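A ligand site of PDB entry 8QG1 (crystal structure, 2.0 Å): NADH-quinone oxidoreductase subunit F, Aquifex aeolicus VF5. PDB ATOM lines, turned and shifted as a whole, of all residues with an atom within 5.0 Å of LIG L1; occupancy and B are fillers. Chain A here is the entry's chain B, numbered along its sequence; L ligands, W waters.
N of Glu 185 sits at hydrogen-bond distance from O3 of LG2 L2.
OE2 of Glu 185 is in hydrogen-bond range of O1 of LIG L1 (2.5 Å).
An oxygen (O9) of LG2 L2 lies within salt-bridge range of the side-chain amino group (NZ) of Lys 76 (2.7 Å).
An oxygen (O14) of LIG L1 is in hydrogen-bond range of the backbone carbonyl oxygen (O) of Gly 68, 2.9 Å away.
An oxygen (O8) of LG2 L2 lies within hydrogen-bond range of the backbone NH (N) of Gly 67 (2.8 Å).
The side-chain amino group of Lys 76 sits at hydrogen-bond distance from an oxygen (O2) of LIG L1, 2.8 Å away.
O4 of LG2 L2 sits at hydrogen-bond distance from O9 of LIG L1.
The backbone carbonyl oxygen (O) of Val 218 is in hydrogen-bond range of the side-chain amino group (NZ) of Lys 76, at 2.7 Å.
Residues that only touch LIG L1: Phe 71, Ala 69, Tyr 205, Pro 206, Val 207 and Leu 297.
Of the 18 residues printed, 9 come within 4 Å of LIG L1.
Water W7 lies within hydrogen-bond range of O13 of LIG L1 (2.5 Å) and OE1 of Glu 97 (2.6 Å).
Water W1 bridges an oxygen (O12) of LIG L1 (2.7 Å) and the backbone carbonyl oxygen (O) of Gly 394 (3.0 Å).
Water W10 bridges the side-chain hydroxyl of Tyr 180 (2.7 Å) and an oxygen (O12) of LIG L1 (2.7 Å).
Water W8 bridges N3 of LIG L1 (2.7 Å) and OH of Tyr 205 (3.0 Å).
Water W11 bridges the side-chain hydroxyl of Tyr 205 and an oxygen (O6) of LIG L1.
Water W5 lies within hydrogen-bond range of the side-chain carboxylate (OE2) of Glu 185, an oxygen (O9) of LIG L1 and the side-chain carboxylate (OE2) of Glu 184.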
ATOM      1  N   GLY A  67       8.445  13.375  -1.270  1.00  0.00           N
ATOM      2  CA  GLY A  67       9.072  12.403  -0.396  1.00  0.00           C
ATOM      3  C   GLY A  67       9.346  11.066  -1.106  1.00  0.00           C
ATOM      4  O   GLY A  67       9.872  10.148  -0.490  1.00  0.00           O
ATOM      5  N   GLY A  68       8.954  10.975  -2.395  1.00  0.00           N
ATOM      6  CA  GLY A  68       9.349   9.844  -3.206  1.00  0.00           C
ATOM      7  C   GLY A  68       8.244   9.301  -4.108  1.00  0.00           C
ATOM      8  O   GLY A  68       8.554   8.789  -5.182  1.00  0.00           O
ATOM      9  N   ALA A  69       6.974   9.382  -3.676  1.00  0.00           N
ATOM     10  CA  ALA A  69       5.862   8.686  -4.340  1.00  0.00           C
ATOM     11  C   ALA A  69       5.002   9.630  -5.189  1.00  0.00           C
ATOM     12  O   ALA A  69       4.147   9.154  -5.937  1.00  0.00           O
ATOM     13  CB  ALA A  69       5.020   7.971  -3.315  1.00  0.00           C
ATOM     14  N   PHE A  71       2.437  11.694  -4.681  1.00  0.00           N
ATOM     15  CA  PHE A  71       0.996  11.734  -4.531  1.00  0.00           C
ATOM     16  C   PHE A  71       0.510  13.185  -4.466  1.00  0.00           C
ATOM     17  O   PHE A  71       1.147  14.011  -3.824  1.00  0.00           O
ATOM     18  CB  PHE A  71       0.553  10.909  -3.313  1.00  0.00           C
ATOM     19  CG  PHE A  71      -0.943  10.742  -3.180  1.00  0.00           C
ATOM     20  CD1 PHE A  71      -1.707  11.697  -2.537  1.00  0.00           C
ATOM     21  CD2 PHE A  71      -1.593   9.662  -3.745  1.00  0.00           C
ATOM     22  CE1 PHE A  71      -3.086  11.563  -2.423  1.00  0.00           C
ATOM     23  CE2 PHE A  71      -2.967   9.524  -3.658  1.00  0.00           C
ATOM     24  CZ  PHE A  71      -3.716  10.470  -2.990  1.00  0.00           C
ATOM     25  N   LYS A  76      -4.560  14.543  -0.967  1.00  0.00           N
ATOM     26  CA  LYS A  76      -4.276  13.894   0.298  1.00  0.00           C
ATOM     27  C   LYS A  76      -5.004  14.646   1.405  1.00  0.00           C
ATOM     28  O   LYS A  76      -5.634  14.026   2.260  1.00  0.00           O
ATOM     29  CB  LYS A  76      -2.776  13.806   0.579  1.00  0.00           C
ATOM     30  CG  LYS A  76      -2.411  12.912   1.749  1.00  0.00           C
ATOM     31  CD  LYS A  76      -0.963  12.970   2.182  1.00  0.00           C
ATOM     32  CE  LYS A  76       0.016  12.497   1.126  1.00  0.00           C
ATOM     33  NZ  LYS A  76       1.397  12.404   1.670  1.00  0.00           N
ATOM     34  N   PHE A  79      -8.786  14.021   1.454  1.00  0.00           N
ATOM     35  CA  PHE A  79      -9.097  12.718   2.031  1.00  0.00           C
ATOM     36  C   PHE A  79      -9.145  12.812   3.556  1.00  0.00           C
ATOM     37  O   PHE A  79     -10.023  12.217   4.180  1.00  0.00           O
ATOM     38  CB  PHE A  79      -8.112  11.642   1.557  1.00  0.00           C
ATOM     39  CG  PHE A  79      -8.425  11.027   0.219  1.00  0.00           C
ATOM     40  CD1 PHE A  79      -9.547  10.227   0.048  1.00  0.00           C
ATOM     41  CD2 PHE A  79      -7.576  11.206  -0.867  1.00  0.00           C
ATOM     42  CE1 PHE A  79      -9.830   9.641  -1.179  1.00  0.00           C
ATOM     43  CE2 PHE A  79      -7.858  10.620  -2.094  1.00  0.00           C
ATOM     44  CZ  PHE A  79      -8.980   9.842  -2.254  1.00  0.00           C
ATOM     45  N   GLU A  97      17.490   7.973   2.873  1.00  0.00           N
ATOM     46  CA  GLU A  97      17.790   7.195   1.681  1.00  0.00           C
ATOM     47  C   GLU A  97      19.147   7.624   1.114  1.00  0.00           C
ATOM     48  O   GLU A  97      19.405   8.826   0.999  1.00  0.00           O
ATOM     49  CB  GLU A  97      16.707   7.370   0.609  1.00  0.00           C
ATOM     50  CG  GLU A  97      16.844   6.374  -0.539  1.00  0.00           C
ATOM     51  CD  GLU A  97      15.812   6.488  -1.644  1.00  0.00           C
ATOM     52  OE1 GLU A  97      14.761   7.136  -1.426  1.00  0.00           O
ATOM     53  OE2 GLU A  97      16.064   5.931  -2.738  1.00  0.00           O
ATOM     54  N   TYR A 180      15.989   3.669   9.065  1.00  0.00           N
ATOM     55  CA  TYR A 180      15.521   4.187   7.784  1.00  0.00           C
ATOM     56  C   TYR A 180      14.014   3.966   7.625  1.00  0.00           C
ATOM     57  O   TYR A 180      13.339   4.792   7.016  1.00  0.00           O
ATOM     58  CB  TYR A 180      16.262   3.517   6.617  1.00  0.00           C
ATOM     59  CG  TYR A 180      15.665   3.748   5.251  1.00  0.00           C
ATOM     60  CD1 TYR A 180      15.654   4.999   4.663  1.00  0.00           C
ATOM     61  CD2 TYR A 180      15.106   2.700   4.538  1.00  0.00           C
ATOM     62  CE1 TYR A 180      15.096   5.208   3.416  1.00  0.00           C
ATOM     63  CE2 TYR A 180      14.541   2.898   3.284  1.00  0.00           C
ATOM     64  CZ  TYR A 180      14.533   4.152   2.719  1.00  0.00           C
ATOM     65  OH  TYR A 180      13.963   4.333   1.481  1.00  0.00           O
ATOM     66  N   GLU A 184       9.090   5.631   6.406  1.00  0.00           N
ATOM     67  CA  GLU A 184       7.816   5.118   5.918  1.00  0.00           C
ATOM     68  C   GLU A 184       6.749   5.641   6.863  1.00  0.00           C
ATOM     69  O   GLU A 184       6.929   5.579   8.083  1.00  0.00           O
ATOM     70  CB  GLU A 184       7.855   3.590   5.831  1.00  0.00           C
ATOM     71  CG  GLU A 184       6.749   2.981   4.967  1.00  0.00           C
ATOM     72  CD  GLU A 184       5.369   2.855   5.589  1.00  0.00           C
ATOM     73  OE1 GLU A 184       5.252   3.026   6.821  1.00  0.00           O
ATOM     74  OE2 GLU A 184       4.410   2.615   4.831  1.00  0.00           O
ATOM     75  N   GLU A 185       5.648   6.173   6.310  1.00  0.00           N
ATOM     76  CA  GLU A 185       4.784   7.073   7.058  1.00  0.00           C
ATOM     77  C   GLU A 185       4.133   6.374   8.255  1.00  0.00           C
ATOM     78  O   GLU A 185       3.943   6.998   9.293  1.00  0.00           O
ATOM     79  CB  GLU A 185       3.721   7.723   6.161  1.00  0.00           C
ATOM     80  CG  GLU A 185       2.871   6.735   5.378  1.00  0.00           C
ATOM     81  CD  GLU A 185       1.783   7.362   4.524  1.00  0.00           C
ATOM     82  OE1 GLU A 185       1.665   8.623   4.504  1.00  0.00           O
ATOM     83  OE2 GLU A 185       1.048   6.579   3.886  1.00  0.00           O
ATOM     84  N   TYR A 205      -5.022   4.234   5.026  1.00  0.00           N
ATOM     85  CA  TYR A 205      -3.961   5.223   4.919  1.00  0.00           C
ATOM     86  C   TYR A 205      -4.038   6.146   6.125  1.00  0.00           C
ATOM     87  O   TYR A 205      -5.083   6.236   6.779  1.00  0.00           O
ATOM     88  CB  TYR A 205      -4.058   5.970   3.573  1.00  0.00           C
ATOM     89  CG  TYR A 205      -3.734   5.098   2.393  1.00  0.00           C
ATOM     90  CD1 TYR A 205      -2.419   4.920   1.969  1.00  0.00           C
ATOM     91  CD2 TYR A 205      -4.721   4.377   1.742  1.00  0.00           C
ATOM     92  CE1 TYR A 205      -2.112   4.094   0.895  1.00  0.00           C
ATOM     93  CE2 TYR A 205      -4.432   3.544   0.680  1.00  0.00           C
ATOM     94  CZ  TYR A 205      -3.121   3.397   0.258  1.00  0.00           C
ATOM     95  OH  TYR A 205      -2.845   2.566  -0.807  1.00  0.00           O
ATOM     96  N   PRO A 206      -2.930   6.839   6.490  1.00  0.00           N
ATOM     97  CA  PRO A 206      -2.918   7.716   7.661  1.00  0.00           C
ATOM     98  C   PRO A 206      -4.059   8.719   7.687  1.00  0.00           C
ATOM     99  O   PRO A 206      -4.587   9.024   8.758  1.00  0.00           O
ATOM    100  CB  PRO A 206      -1.554   8.412   7.551  1.00  0.00           C
ATOM    101  CG  PRO A 206      -0.695   7.389   6.871  1.00  0.00           C
ATOM    102  CD  PRO A 206      -1.612   6.785   5.831  1.00  0.00           C
ATOM    103  N   VAL A 207      -4.470   9.210   6.501  1.00  0.00           N
ATOM    104  CA  VAL A 207      -5.495  10.243   6.400  1.00  0.00           C
ATOM    105  C   VAL A 207      -6.838   9.726   6.924  1.00  0.00           C
ATOM    106  O   VAL A 207      -7.691  10.528   7.281  1.00  0.00           O
ATOM    107  CB  VAL A 207      -5.623  10.790   4.961  1.00  0.00           C
ATOM    108  CG1 VAL A 207      -4.406  11.614   4.572  1.00  0.00           C
ATOM    109  CG2 VAL A 207      -5.894   9.690   3.947  1.00  0.00           C
ATOM    110  N   VAL A 218       0.648  12.959   6.586  1.00  0.00           N
ATOM    111  CA  VAL A 218       2.100  12.965   6.584  1.00  0.00           C
ATOM    112  C   VAL A 218       2.570  13.582   5.270  1.00  0.00           C
ATOM    113  O   VAL A 218       2.155  13.143   4.200  1.00  0.00           O
ATOM    114  CB  VAL A 218       2.694  11.559   6.758  1.00  0.00           C
ATOM    115  CG1 VAL A 218       4.213  11.613   6.805  1.00  0.00           C
ATOM    116  CG2 VAL A 218       2.125  10.842   7.973  1.00  0.00           C
ATOM    117  N   LEU A 297      16.678   3.455  -5.416  1.00  0.00           N
ATOM    118  CA  LEU A 297      15.414   3.079  -6.023  1.00  0.00           C
ATOM    119  C   LEU A 297      15.606   2.590  -7.465  1.00  0.00           C
ATOM    120  O   LEU A 297      15.101   1.517  -7.814  1.00  0.00           O
ATOM    121  CB  LEU A 297      14.468   4.277  -5.929  1.00  0.00           C
ATOM    122  CG  LEU A 297      13.046   4.055  -6.435  1.00  0.00           C
ATOM    123  CD1 LEU A 297      12.297   3.058  -5.548  1.00  0.00           C
ATOM    124  CD2 LEU A 297      12.292   5.371  -6.511  1.00  0.00           C
ATOM    125  N   GLY A 318      11.006   9.494  -8.234  1.00  0.00           N
ATOM    126  CA  GLY A 318      11.576   9.426  -6.903  1.00  0.00           C
ATOM    127  C   GLY A 318      11.608  10.792  -6.219  1.00  0.00           C
ATOM    128  O   GLY A 318      10.633  11.521  -6.261  1.00  0.00           O
ATOM    129  N   GLY A 394       6.681  -0.407   1.222  1.00  0.00           N
ATOM    130  CA  GLY A 394       7.394  -0.188  -0.026  1.00  0.00           C
ATOM    131  C   GLY A 394       8.841  -0.655   0.001  1.00  0.00           C
ATOM    132  O   GLY A 394       9.421  -0.855  -1.059  1.00  0.00           O
ATOM    133  N   VAL A 398      10.763  -2.676  -3.163  1.00  0.00           N
ATOM    134  CA  VAL A 398      11.812  -2.107  -3.997  1.00  0.00           C
ATOM    135  C   VAL A 398      13.214  -2.587  -3.613  1.00  0.00           C
ATOM    136  O   VAL A 398      14.181  -2.222  -4.288  1.00  0.00           O
ATOM    137  CB  VAL A 398      11.755  -0.561  -4.031  1.00  0.00           C
ATOM    138  CG1 VAL A 398      10.415  -0.062  -4.530  1.00  0.00           C
ATOM    139  CG2 VAL A 398      12.116   0.077  -2.702  1.00  0.00           C
HETATM  140  N1  LIG L   1      -5.745   7.370  -0.244  1.00  0.00           N
HETATM  141  C1  LIG L   1      -5.110   8.254   0.543  1.00  0.00           C
HETATM  142  N2  LIG L   1      -3.803   8.530   0.605  1.00  0.00           N
HETATM  143  C2  LIG L   1      -3.109   7.781  -0.261  1.00  0.00           C
HETATM  144  C3  LIG L   1      -3.624   6.830  -1.139  1.00  0.00           C
HETATM  145  C4  LIG L   1      -5.015   6.626  -1.111  1.00  0.00           C
HETATM  146  N3  LIG L   1      -5.653   5.726  -1.860  1.00  0.00           N
HETATM  147  N4  LIG L   1      -2.614   6.265  -1.900  1.00  0.00           N
HETATM  148  C5  LIG L   1      -1.526   6.875  -1.483  1.00  0.00           C
HETATM  149  N5  LIG L   1      -1.755   7.803  -0.488  1.00  0.00           N
HETATM  150  C6  LIG L   1      -0.750   8.579   0.209  1.00  0.00           C
HETATM  151  C7  LIG L   1       0.026   7.792   1.267  1.00  0.00           C
HETATM  152  O1  LIG L   1      -0.641   7.845   2.536  1.00  0.00           O
HETATM  153  C8  LIG L   1       1.373   8.532   1.264  1.00  0.00           C
HETATM  154  O2  LIG L   1       1.381   9.651   2.153  1.00  0.00           O
HETATM  155  O3  LIG L   1       0.202   9.035  -0.737  1.00  0.00           O
HETATM  156  C9  LIG L   1       1.541   8.947  -0.202  1.00  0.00           C
HETATM  157  C10 LIG L   1       2.355   8.002  -1.047  1.00  0.00           C
HETATM  158  O4  LIG L   1       1.864   6.660  -0.818  1.00  0.00           O
HETATM  159  P1  LIG L   1       2.456   5.345  -1.515  1.00  0.00           P
HETATM  160  O5  LIG L   1       2.250   5.432  -2.983  1.00  0.00           O
HETATM  161  O6  LIG L   1       1.836   4.210  -0.795  1.00  0.00           O
HETATM  162  O7  LIG L   1       4.020   5.424  -1.208  1.00  0.00           O
HETATM  163  P2  LIG L   1       4.899   5.151   0.101  1.00  0.00           P
HETATM  164  O8  LIG L   1       4.880   3.698   0.413  1.00  0.00           O
HETATM  165  O9  LIG L   1       4.557   6.113   1.171  1.00  0.00           O
HETATM  166  O10 LIG L   1       6.362   5.576  -0.380  1.00  0.00           O
HETATM  167  C11 LIG L   1       7.008   4.926  -1.495  1.00  0.00           C
HETATM  168  O11 LIG L   1       9.275   5.619  -0.983  1.00  0.00           O
HETATM  169  O12 LIG L   1      10.643   3.770  -1.486  1.00  0.00           O
HETATM  170  C12 LIG L   1      10.463   5.177  -1.626  1.00  0.00           C
HETATM  171  O13 LIG L   1      10.561   6.872  -3.411  1.00  0.00           O
HETATM  172  C13 LIG L   1      10.263   5.515  -3.107  1.00  0.00           C
HETATM  173  O14 LIG L   1       8.227   5.993  -4.367  1.00  0.00           O
HETATM  174  C14 LIG L   1       8.772   5.259  -3.287  1.00  0.00           C
HETATM  175  C15 LIG L   1       8.199   5.724  -1.950  1.00  0.00           C
HETATM  176  N1  LG2 L   2       9.048  10.136   2.901  1.00  0.00           N
HETATM  177  C1  LG2 L   2       9.728  11.207   3.423  1.00  0.00           C
HETATM  178  O1  LG2 L   2       9.235  12.358   3.442  1.00  0.00           O
HETATM  179  N2  LG2 L   2      10.966  10.999   4.042  1.00  0.00           N
HETATM  180  C2  LG2 L   2      11.593   9.783   4.225  1.00  0.00           C
HETATM  181  O2  LG2 L   2      12.669   9.736   4.827  1.00  0.00           O
HETATM  182  C3  LG2 L   2      10.858   8.636   3.682  1.00  0.00           C
HETATM  183  N3  LG2 L   2      11.353   7.434   3.845  1.00  0.00           N
HETATM  184  C4  LG2 L   2      10.621   6.354   3.359  1.00  0.00           C
HETATM  185  C5  LG2 L   2      11.129   5.063   3.552  1.00  0.00           C
HETATM  186  C6  LG2 L   2      10.435   3.949   3.077  1.00  0.00           C
HETATM  187  C7  LG2 L   2      11.026   2.567   3.277  1.00  0.00           C
HETATM  188  C8  LG2 L   2       9.218   4.118   2.409  1.00  0.00           C
HETATM  189  C9  LG2 L   2       8.506   2.930   1.804  1.00  0.00           C
HETATM  190  C10 LG2 L   2       8.707   5.389   2.219  1.00  0.00           C
HETATM  191  C11 LG2 L   2       9.397   6.513   2.684  1.00  0.00           C
HETATM  192  N4  LG2 L   2       8.899   7.838   2.532  1.00  0.00           N
HETATM  193  C12 LG2 L   2       9.586   8.924   3.023  1.00  0.00           C
HETATM  194  C13 LG2 L   2       7.592   8.074   1.909  1.00  0.00           C
HETATM  195  C14 LG2 L   2       6.535   8.196   2.993  1.00  0.00           C
HETATM  196  O3  LG2 L   2       6.052   6.899   3.348  1.00  0.00           O
HETATM  197  C15 LG2 L   2       5.383   9.078   2.511  1.00  0.00           C
HETATM  198  O4  LG2 L   2       4.994   8.679   1.194  1.00  0.00           O
HETATM  199  C16 LG2 L   2       5.712  10.576   2.484  1.00  0.00           C
HETATM  200  O5  LG2 L   2       6.312  10.999   3.707  1.00  0.00           O
HETATM  201  C17 LG2 L   2       4.477  11.402   2.206  1.00  0.00           C
HETATM  202  O6  LG2 L   2       4.826  12.797   2.022  1.00  0.00           O
HETATM  203  P1  LG2 L   2       4.710  13.439   0.536  1.00  0.00           P
HETATM  204  O7  LG2 L   2       4.823  14.918   0.812  1.00  0.00           O
HETATM  205  O8  LG2 L   2       5.856  12.881  -0.280  1.00  0.00           O
HETATM  206  O9  LG2 L   2       3.355  13.077  -0.047  1.00  0.00           O
HETATM  207  O   HOH W   1       8.854   1.875  -2.114  1.00  0.00           O
HETATM  208  O   HOH W   2       4.869   1.746  -1.774  1.00  0.00           O
HETATM  209  O   HOH W   3      -8.342   6.518   0.208  1.00  0.00           O
HETATM  210  O   HOH W   4       5.004   1.837   2.235  1.00  0.00           O
HETATM  211  O   HOH W   5       2.463   4.372   2.723  1.00  0.00           O
HETATM  212  O   HOH W   6      -1.821   4.459  -4.043  1.00  0.00           O
HETATM  213  O   HOH W   7      12.917   7.633  -3.263  1.00  0.00           O
HETATM  214  O   HOH W   8      -4.137   3.910  -3.211  1.00  0.00           O
HETATM  215  O   HOH W   9      -2.517   9.398   3.246  1.00  0.00           O
HETATM  216  O   HOH W  10      12.853   2.701  -0.313  1.00  0.00           O
HETATM  217  O   HOH W  11      -0.434   3.070  -2.522  1.00  0.00           O
